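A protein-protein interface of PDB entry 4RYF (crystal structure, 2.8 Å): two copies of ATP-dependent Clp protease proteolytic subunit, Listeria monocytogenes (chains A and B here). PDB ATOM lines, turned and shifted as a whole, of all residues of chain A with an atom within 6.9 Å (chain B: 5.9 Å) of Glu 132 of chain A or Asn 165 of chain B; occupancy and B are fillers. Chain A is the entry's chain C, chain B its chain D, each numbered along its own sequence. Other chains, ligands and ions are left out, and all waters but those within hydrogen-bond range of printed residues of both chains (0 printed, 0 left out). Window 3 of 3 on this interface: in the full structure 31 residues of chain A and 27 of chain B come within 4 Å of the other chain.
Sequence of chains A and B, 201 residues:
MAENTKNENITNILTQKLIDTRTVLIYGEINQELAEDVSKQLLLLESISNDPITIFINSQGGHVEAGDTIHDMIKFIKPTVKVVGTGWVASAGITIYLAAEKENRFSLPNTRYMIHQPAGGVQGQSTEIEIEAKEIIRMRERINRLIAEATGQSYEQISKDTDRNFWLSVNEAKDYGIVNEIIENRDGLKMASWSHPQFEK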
ATOM      1  N   GLY A 121      19.145  -6.110 -16.523  1.00  0.00           N
ATOM      2  CA  GLY A 121      17.975  -6.969 -16.653  1.00  0.00           C
ATOM      3  C   GLY A 121      16.903  -6.346 -17.523  1.00  0.00           C
ATOM      4  O   GLY A 121      16.749  -5.126 -17.552  1.00  0.00           O
ATOM      5  N   VAL A 122      16.175  -7.186 -18.253  1.00  0.00           N
ATOM      6  CA  VAL A 122      15.017  -6.733 -19.018  1.00  0.00           C
ATOM      7  C   VAL A 122      13.890  -7.739 -18.904  1.00  0.00           C
ATOM      8  O   VAL A 122      14.126  -8.947 -18.879  1.00  0.00           O
ATOM      9  CB  VAL A 122      15.290  -6.563 -20.529  1.00  0.00           C
ATOM     10  CG1 VAL A 122      14.669  -5.263 -21.019  1.00  0.00           C
ATOM     11  CG2 VAL A 122      16.777  -6.622 -20.856  1.00  0.00           C
ATOM     12  N   SER A 126       9.940  -9.422 -26.921  1.00  0.00           N
ATOM     13  CA  SER A 126      11.193  -9.564 -27.668  1.00  0.00           C
ATOM     14  C   SER A 126      11.753  -8.209 -28.071  1.00  0.00           C
ATOM     15  O   SER A 126      12.921  -7.921 -27.814  1.00  0.00           O
ATOM     16  CB  SER A 126      10.985 -10.399 -28.930  1.00  0.00           C
ATOM     17  OG  SER A 126      10.619 -11.726 -28.619  1.00  0.00           O
ATOM     18  N   THR A 127      10.908  -7.389 -28.695  1.00  0.00           N
ATOM     19  CA  THR A 127      11.280  -6.053 -29.161  1.00  0.00           C
ATOM     20  C   THR A 127      11.933  -5.234 -28.049  1.00  0.00           C
ATOM     21  O   THR A 127      12.982  -4.623 -28.259  1.00  0.00           O
ATOM     22  CB  THR A 127      10.058  -5.305 -29.743  1.00  0.00           C
ATOM     23  OG1 THR A 127       9.571  -6.011 -30.891  1.00  0.00           O
ATOM     24  CG2 THR A 127      10.422  -3.885 -30.153  1.00  0.00           C
ATOM     25  N   GLU A 128      11.314  -5.244 -26.869  1.00  0.00           N
ATOM     26  CA  GLU A 128      11.835  -4.528 -25.705  1.00  0.00           C
ATOM     27  C   GLU A 128      13.178  -5.097 -25.238  1.00  0.00           C
ATOM     28  O   GLU A 128      14.107  -4.340 -24.943  1.00  0.00           O
ATOM     29  CB  GLU A 128      10.807  -4.533 -24.569  1.00  0.00           C
ATOM     30  CG  GLU A 128       9.557  -3.716 -24.876  1.00  0.00           C
ATOM     31  CD  GLU A 128       8.402  -3.984 -23.925  1.00  0.00           C
ATOM     32  OE1 GLU A 128       8.116  -5.164 -23.620  1.00  0.00           O
ATOM     33  OE2 GLU A 128       7.758  -3.005 -23.493  1.00  0.00           O
ATOM     34  N   ILE A 129      13.271  -6.427 -25.192  1.00  0.00           N
ATOM     35  CA  ILE A 129      14.500  -7.132 -24.813  1.00  0.00           C
ATOM     36  C   ILE A 129      15.617  -6.857 -25.821  1.00  0.00           C
ATOM     37  O   ILE A 129      16.745  -6.533 -25.439  1.00  0.00           O
ATOM     38  CB  ILE A 129      14.257  -8.655 -24.685  1.00  0.00           C
ATOM     39  CG1 ILE A 129      13.316  -8.945 -23.510  1.00  0.00           C
ATOM     40  CG2 ILE A 129      15.571  -9.410 -24.519  1.00  0.00           C
ATOM     41  CD1 ILE A 129      12.687 -10.323 -23.532  1.00  0.00           C
ATOM     42  N   GLU A 130      15.281  -6.983 -27.104  1.00  0.00           N
ATOM     43  CA  GLU A 130      16.195  -6.719 -28.214  1.00  0.00           C
ATOM     44  C   GLU A 130      16.783  -5.306 -28.139  1.00  0.00           C
ATOM     45  O   GLU A 130      17.993  -5.126 -28.283  1.00  0.00           O
ATOM     46  CB  GLU A 130      15.458  -6.926 -29.540  1.00  0.00           C
ATOM     47  CG  GLU A 130      16.341  -6.990 -30.777  1.00  0.00           C
ATOM     48  CD  GLU A 130      15.540  -7.134 -32.062  1.00  0.00           C
ATOM     49  OE1 GLU A 130      14.359  -7.552 -32.001  1.00  0.00           O
ATOM     50  OE2 GLU A 130      16.095  -6.829 -33.140  1.00  0.00           O
ATOM     51  N   ILE A 131      15.916  -4.320 -27.903  1.00  0.00           N
ATOM     52  CA  ILE A 131      16.313  -2.914 -27.780  1.00  0.00           C
ATOM     53  C   ILE A 131      17.322  -2.709 -26.651  1.00  0.00           C
ATOM     54  O   ILE A 131      18.326  -2.011 -26.824  1.00  0.00           O
ATOM     55  CB  ILE A 131      15.080  -1.994 -27.600  1.00  0.00           C
ATOM     56  CG1 ILE A 131      14.441  -1.715 -28.962  1.00  0.00           C
ATOM     57  CG2 ILE A 131      15.452  -0.680 -26.918  1.00  0.00           C
ATOM     58  CD1 ILE A 131      13.031  -1.177 -28.888  1.00  0.00           C
ATOM     59  N   GLU A 132      17.060  -3.337 -25.508  1.00  0.00           N
ATOM     60  CA  GLU A 132      17.903  -3.185 -24.333  1.00  0.00           C
ATOM     61  C   GLU A 132      19.216  -3.954 -24.488  1.00  0.00           C
ATOM     62  O   GLU A 132      20.250  -3.542 -23.955  1.00  0.00           O
ATOM     63  CB  GLU A 132      17.145  -3.630 -23.084  1.00  0.00           C
ATOM     64  CG  GLU A 132      17.117  -2.591 -21.967  1.00  0.00           C
ATOM     65  CD  GLU A 132      16.418  -1.289 -22.356  1.00  0.00           C
ATOM     66  OE1 GLU A 132      16.855  -0.224 -21.868  1.00  0.00           O
ATOM     67  OE2 GLU A 132      15.442  -1.316 -23.144  1.00  0.00           O
ATOM     68  N   ALA A 133      19.166  -5.059 -25.232  1.00  0.00           N
ATOM     69  CA  ALA A 133      20.358  -5.839 -25.564  1.00  0.00           C
ATOM     70  C   ALA A 133      21.336  -5.025 -26.408  1.00  0.00           C
ATOM     71  O   ALA A 133      22.516  -4.938 -26.072  1.00  0.00           O
ATOM     72  CB  ALA A 133      19.978  -7.124 -26.277  1.00  0.00           C
ATOM     73  N   LYS A 134      20.840  -4.424 -27.492  1.00  0.00           N
ATOM     74  CA  LYS A 134      21.648  -3.527 -28.319  1.00  0.00           C
ATOM     75  C   LYS A 134      22.292  -2.436 -27.473  1.00  0.00           C
ATOM     76  O   LYS A 134      23.450  -2.068 -27.687  1.00  0.00           O
ATOM     77  CB  LYS A 134      20.800  -2.895 -29.423  1.00  0.00           C
ATOM     78  CG  LYS A 134      20.668  -3.764 -30.659  1.00  0.00           C
ATOM     79  CD  LYS A 134      19.576  -3.265 -31.589  1.00  0.00           C
ATOM     80  CE  LYS A 134      19.342  -4.255 -32.719  1.00  0.00           C
ATOM     81  NZ  LYS A 134      18.000  -4.090 -33.339  1.00  0.00           N
ATOM     82  N   GLU A 135      21.536  -1.945 -26.497  1.00  0.00           N
ATOM     83  CA  GLU A 135      21.982  -0.859 -25.646  1.00  0.00           C
ATOM     84  C   GLU A 135      23.112  -1.272 -24.698  1.00  0.00           C
ATOM     85  O   GLU A 135      24.084  -0.527 -24.538  1.00  0.00           O
ATOM     86  CB  GLU A 135      20.791  -0.271 -24.888  1.00  0.00           C
ATOM     87  CG  GLU A 135      20.909   1.211 -24.566  1.00  0.00           C
ATOM     88  CD  GLU A 135      21.602   2.030 -25.645  1.00  0.00           C
ATOM     89  OE1 GLU A 135      21.315   1.837 -26.850  1.00  0.00           O
ATOM     90  OE2 GLU A 135      22.435   2.886 -25.281  1.00  0.00           O
ATOM     91  N   ILE A 136      22.999  -2.452 -24.091  1.00  0.00           N
ATOM     92  CA  ILE A 136      24.052  -2.936 -23.191  1.00  0.00           C
ATOM     93  C   ILE A 136      25.324  -3.373 -23.945  1.00  0.00           C
ATOM     94  O   ILE A 136      26.430  -3.260 -23.410  1.00  0.00           O
ATOM     95  CB  ILE A 136      23.542  -4.004 -22.185  1.00  0.00           C
ATOM     96  CG1 ILE A 136      24.488  -4.095 -20.976  1.00  0.00           C
ATOM     97  CG2 ILE A 136      23.331  -5.357 -22.860  1.00  0.00           C
ATOM     98  CD1 ILE A 136      23.893  -4.758 -19.750  1.00  0.00           C
ATOM     99  N   ILE A 137      25.165  -3.851 -25.181  1.00  0.00           N
ATOM    100  CA  ILE A 137      26.311  -4.162 -26.050  1.00  0.00           C
ATOM    101  C   ILE A 137      27.113  -2.889 -26.340  1.00  0.00           C
ATOM    102  O   ILE A 137      28.344  -2.887 -26.246  1.00  0.00           O
ATOM    103  CB  ILE A 137      25.884  -4.836 -27.384  1.00  0.00           C
ATOM    104  CG1 ILE A 137      25.137  -6.160 -27.143  1.00  0.00           C
ATOM    105  CG2 ILE A 137      27.081  -5.052 -28.302  1.00  0.00           C
ATOM    106  CD1 ILE A 137      25.890  -7.205 -26.343  1.00  0.00           C
ATOM    107  N   ARG B 112      24.266   8.954 -22.679  1.00  0.00           N
ATOM    108  CA  ARG B 112      23.299   8.425 -23.630  1.00  0.00           C
ATOM    109  C   ARG B 112      21.920   9.024 -23.384  1.00  0.00           C
ATOM    110  O   ARG B 112      21.621   9.503 -22.288  1.00  0.00           O
ATOM    111  CB  ARG B 112      23.281   6.891 -23.637  1.00  0.00           C
ATOM    112  CG  ARG B 112      22.831   6.230 -22.348  1.00  0.00           C
ATOM    113  CD  ARG B 112      23.155   4.747 -22.383  1.00  0.00           C
ATOM    114  NE  ARG B 112      22.809   4.092 -21.125  1.00  0.00           N
ATOM    115  CZ  ARG B 112      21.934   3.097 -21.004  1.00  0.00           C
ATOM    116  NH1 ARG B 112      21.689   2.579 -19.810  1.00  0.00           N
ATOM    117  NH2 ARG B 112      21.314   2.606 -22.067  1.00  0.00           N
ATOM    118  N   MET B 114      17.535   8.963 -24.217  1.00  0.00           N
ATOM    119  CA  MET B 114      16.401   8.099 -24.505  1.00  0.00           C
ATOM    120  C   MET B 114      15.073   8.831 -24.439  1.00  0.00           C
ATOM    121  O   MET B 114      14.749   9.477 -23.440  1.00  0.00           O
ATOM    122  CB  MET B 114      16.394   6.884 -23.575  1.00  0.00           C
ATOM    123  CG  MET B 114      15.482   5.754 -24.027  1.00  0.00           C
ATOM    124  SD  MET B 114      13.834   5.839 -23.300  1.00  0.00           S
ATOM    125  CE  MET B 114      14.148   5.193 -21.660  1.00  0.00           C
ATOM    126  N   ILE B 115      14.314   8.725 -25.522  1.00  0.00           N
ATOM    127  CA  ILE B 115      12.935   9.187 -25.545  1.00  0.00           C
ATOM    128  C   ILE B 115      12.012   7.992 -25.769  1.00  0.00           C
ATOM    129  O   ILE B 115      12.370   7.042 -26.474  1.00  0.00           O
ATOM    130  CB  ILE B 115      12.696  10.294 -26.601  1.00  0.00           C
ATOM    131  CG1 ILE B 115      13.178   9.854 -27.993  1.00  0.00           C
ATOM    132  CG2 ILE B 115      13.377  11.587 -26.169  1.00  0.00           C
ATOM    133  CD1 ILE B 115      12.835  10.820 -29.110  1.00  0.00           C
ATOM    134  N   HIS B 116      10.845   8.031 -25.132  1.00  0.00           N
ATOM    135  CA  HIS B 116       9.823   6.999 -25.295  1.00  0.00           C
ATOM    136  C   HIS B 116       8.451   7.587 -24.980  1.00  0.00           C
ATOM    137  O   HIS B 116       8.356   8.709 -24.479  1.00  0.00           O
ATOM    138  CB  HIS B 116      10.118   5.766 -24.418  1.00  0.00           C
ATOM    139  CG  HIS B 116      10.033   6.018 -22.940  1.00  0.00           C
ATOM    140  ND1 HIS B 116      10.342   5.050 -22.006  1.00  0.00           N
ATOM    141  CD2 HIS B 116       9.683   7.120 -22.233  1.00  0.00           C
ATOM    142  CE1 HIS B 116      10.172   5.540 -20.791  1.00  0.00           C
ATOM    143  NE2 HIS B 116       9.772   6.793 -20.900  1.00  0.00           N
ATOM    144  N   ASP B 161       9.320   7.365 -33.709  1.00  0.00           N
ATOM    145  CA  ASP B 161      10.519   6.950 -32.981  1.00  0.00           C
ATOM    146  C   ASP B 161      10.268   6.599 -31.509  1.00  0.00           C
ATOM    147  O   ASP B 161      10.901   5.683 -30.977  1.00  0.00           O
ATOM    148  CB  ASP B 161      11.621   8.010 -33.107  1.00  0.00           C
ATOM    149  CG  ASP B 161      12.263   8.035 -34.493  1.00  0.00           C
ATOM    150  OD1 ASP B 161      12.198   7.017 -35.214  1.00  0.00           O
ATOM    151  OD2 ASP B 161      12.847   9.077 -34.861  1.00  0.00           O
ATOM    152  N   THR B 162       9.344   7.311 -30.861  1.00  0.00           N
ATOM    153  CA  THR B 162       9.027   7.071 -29.445  1.00  0.00           C
ATOM    154  C   THR B 162       8.068   5.897 -29.216  1.00  0.00           C
ATOM    155  O   THR B 162       7.644   5.649 -28.082  1.00  0.00           O
ATOM    156  CB  THR B 162       8.453   8.324 -28.744  1.00  0.00           C
ATOM    157  OG1 THR B 162       7.261   8.752 -29.414  1.00  0.00           O
ATOM    158  CG2 THR B 162       9.463   9.458 -28.730  1.00  0.00           C
ATOM    159  N   ASP B 163       7.731   5.183 -30.290  1.00  0.00           N
ATOM    160  CA  ASP B 163       6.882   3.994 -30.208  1.00  0.00           C
ATOM    161  C   ASP B 163       7.433   2.997 -29.185  1.00  0.00           C
ATOM    162  O   ASP B 163       6.697   2.487 -28.339  1.00  0.00           O
ATOM    163  CB  ASP B 163       6.752   3.338 -31.584  1.00  0.00           C
ATOM    164  CG  ASP B 163       5.749   2.200 -31.599  1.00  0.00           C
ATOM    165  OD1 ASP B 163       6.084   1.132 -32.151  1.00  0.00           O
ATOM    166  OD2 ASP B 163       4.633   2.367 -31.057  1.00  0.00           O
ATOM    167  N   ARG B 164       8.734   2.736 -29.273  1.00  0.00           N
ATOM    168  CA  ARG B 164       9.453   1.947 -28.278  1.00  0.00           C
ATOM    169  C   ARG B 164      10.550   2.814 -27.677  1.00  0.00           C
ATOM    170  O   ARG B 164      10.696   3.980 -28.055  1.00  0.00           O
ATOM    171  CB  ARG B 164      10.072   0.708 -28.926  1.00  0.00           C
ATOM    172  CG  ARG B 164       9.094  -0.206 -29.644  1.00  0.00           C
ATOM    173  CD  ARG B 164       8.331  -1.082 -28.671  1.00  0.00           C
ATOM    174  NE  ARG B 164       7.499  -2.048 -29.379  1.00  0.00           N
ATOM    175  CZ  ARG B 164       6.901  -3.087 -28.809  1.00  0.00           C
ATOM    176  NH1 ARG B 164       7.042  -3.308 -27.507  1.00  0.00           N
ATOM    177  NH2 ARG B 164       6.163  -3.909 -29.543  1.00  0.00           N
ATOM    178  N   ASN B 165      11.318   2.254 -26.744  1.00  0.00           N
ATOM    179  CA  ASN B 165      12.493   2.941 -26.214  1.00  0.00           C
ATOM    180  C   ASN B 165      13.478   3.289 -27.323  1.00  0.00           C
ATOM    181  O   ASN B 165      14.003   2.409 -28.009  1.00  0.00           O
ATOM    182  CB  ASN B 165      13.180   2.105 -25.135  1.00  0.00           C
ATOM    183  CG  ASN B 165      12.460   2.164 -23.804  1.00  0.00           C
ATOM    184  OD1 ASN B 165      11.362   2.715 -23.694  1.00  0.00           O
ATOM    185  ND2 ASN B 165      13.080   1.592 -22.777  1.00  0.00           N
ATOM    186  N   PHE B 166      13.703   4.585 -27.496  1.00  0.00           N
ATOM    187  CA  PHE B 166      14.565   5.098 -28.549  1.00  0.00           C
ATOM    188  C   PHE B 166      15.860   5.591 -27.917  1.00  0.00           C
ATOM    189  O   PHE B 166      15.945   6.731 -27.458  1.00  0.00           O
ATOM    190  CB  PHE B 166      13.839   6.224 -29.297  1.00  0.00           C
ATOM    191  CG  PHE B 166      14.465   6.599 -30.610  1.00  0.00           C
ATOM    192  CD1 PHE B 166      14.435   5.725 -31.693  1.00  0.00           C
ATOM    193  CD2 PHE B 166      15.056   7.848 -30.776  1.00  0.00           C
ATOM    194  CE1 PHE B 166      15.004   6.081 -32.907  1.00  0.00           C
ATOM    195  CE2 PHE B 166      15.624   8.211 -31.987  1.00  0.00           C
ATOM    196  CZ  PHE B 166      15.600   7.326 -33.054  1.00  0.00           C
ATOM    197  N   TRP B 167      16.857   4.710 -27.872  1.00  0.00           N
ATOM    198  CA  TRP B 167      18.154   5.041 -27.288  1.00  0.00           C
ATOM    199  C   TRP B 167      19.071   5.713 -28.300  1.00  0.00           C
ATOM    200  O   TRP B 167      19.161   5.290 -29.456  1.00  0.00           O
ATOM    201  CB  TRP B 167      18.836   3.798 -26.718  1.00  0.00           C
ATOM    202  CG  TRP B 167      18.246   3.315 -25.433  1.00  0.00           C
ATOM    203  CD1 TRP B 167      17.362   2.287 -25.276  1.00  0.00           C
ATOM    204  CD2 TRP B 167      18.495   3.835 -24.119  1.00  0.00           C
ATOM    205  NE1 TRP B 167      17.042   2.134 -23.949  1.00  0.00           N
ATOM    206  CE2 TRP B 167      17.723   3.071 -23.215  1.00  0.00           C
ATOM    207  CE3 TRP B 167      19.294   4.874 -23.617  1.00  0.00           C
ATOM    208  CZ2 TRP B 167      17.722   3.310 -21.836  1.00  0.00           C
ATOM    209  CZ3 TRP B 167      19.293   5.113 -22.244  1.00  0.00           C
ATOM    210  CH2 TRP B 167      18.511   4.332 -21.371  1.00  0.00           C
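Of the 14 printed residues of chain A, 5 touch a printed residue of chain B. Of the 11 printed residues of chain B, 4 touch a printed residue of chain A. Among the printed residues, 9 pairs touch across the chains.
ND1 of His 116 of chain B is in hydrogen-bond range of OD1 of Asn 165 of chain B, 3.1 Å away.
Of the printed residues of chain B, Ile 131 of chain A touches Arg 164 (3.5 Å), Asn 165 (3.6 Å) and Trp 167 (3.9 Å). Asn 165 of chain B touches just these residues of chain A: Ile 131 and Glu 132. Printed residues of chain A within 4 Å of Trp 167 of chain B: Ile 131 (3.9 Å), Glu 132 (3.2 Å) and Glu 135 (3.2 Å). The nearest residue of chain B that does not touch Glu 132 of chain A is Arg 112 of chain B (5.3 Å).
No position is printed for both chains. Of the 9 pairs that touch across the chains among the printed residues, none has its exchanged pair printed and touching as well.
Thr 127 of chain A touches Arg 164 of chain B (CG2 to NE, 3.5 Å). Arg 164 of chain B touches Glu 128 of chain A (NH1 to CG, 3.7 Å). Ile 131 of chain A touches Arg 164 of chain B (CD1 to CB, 3.5 Å). Ile 131 of chain A touches Asn 165 of chain B (CG2 to O, 3.6 Å). Ile 131 of chain A touches Trp 167 of chain B. Glu 132 of chain A touches Asn 165 of chain B. Glu 135 of chain A touches Trp 167 of chain B (OE1 to CB, 3.2 Å).
The side-chain carboxylate of Glu 135 of chain A is in salt-bridge range of the guanidinium group of Arg 112 of chain B (3.4 Å). OE1 of Glu 132 of chain A lies within hydrogen-bond range of NE1 of Trp 167 of chain B (3.2 Å).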
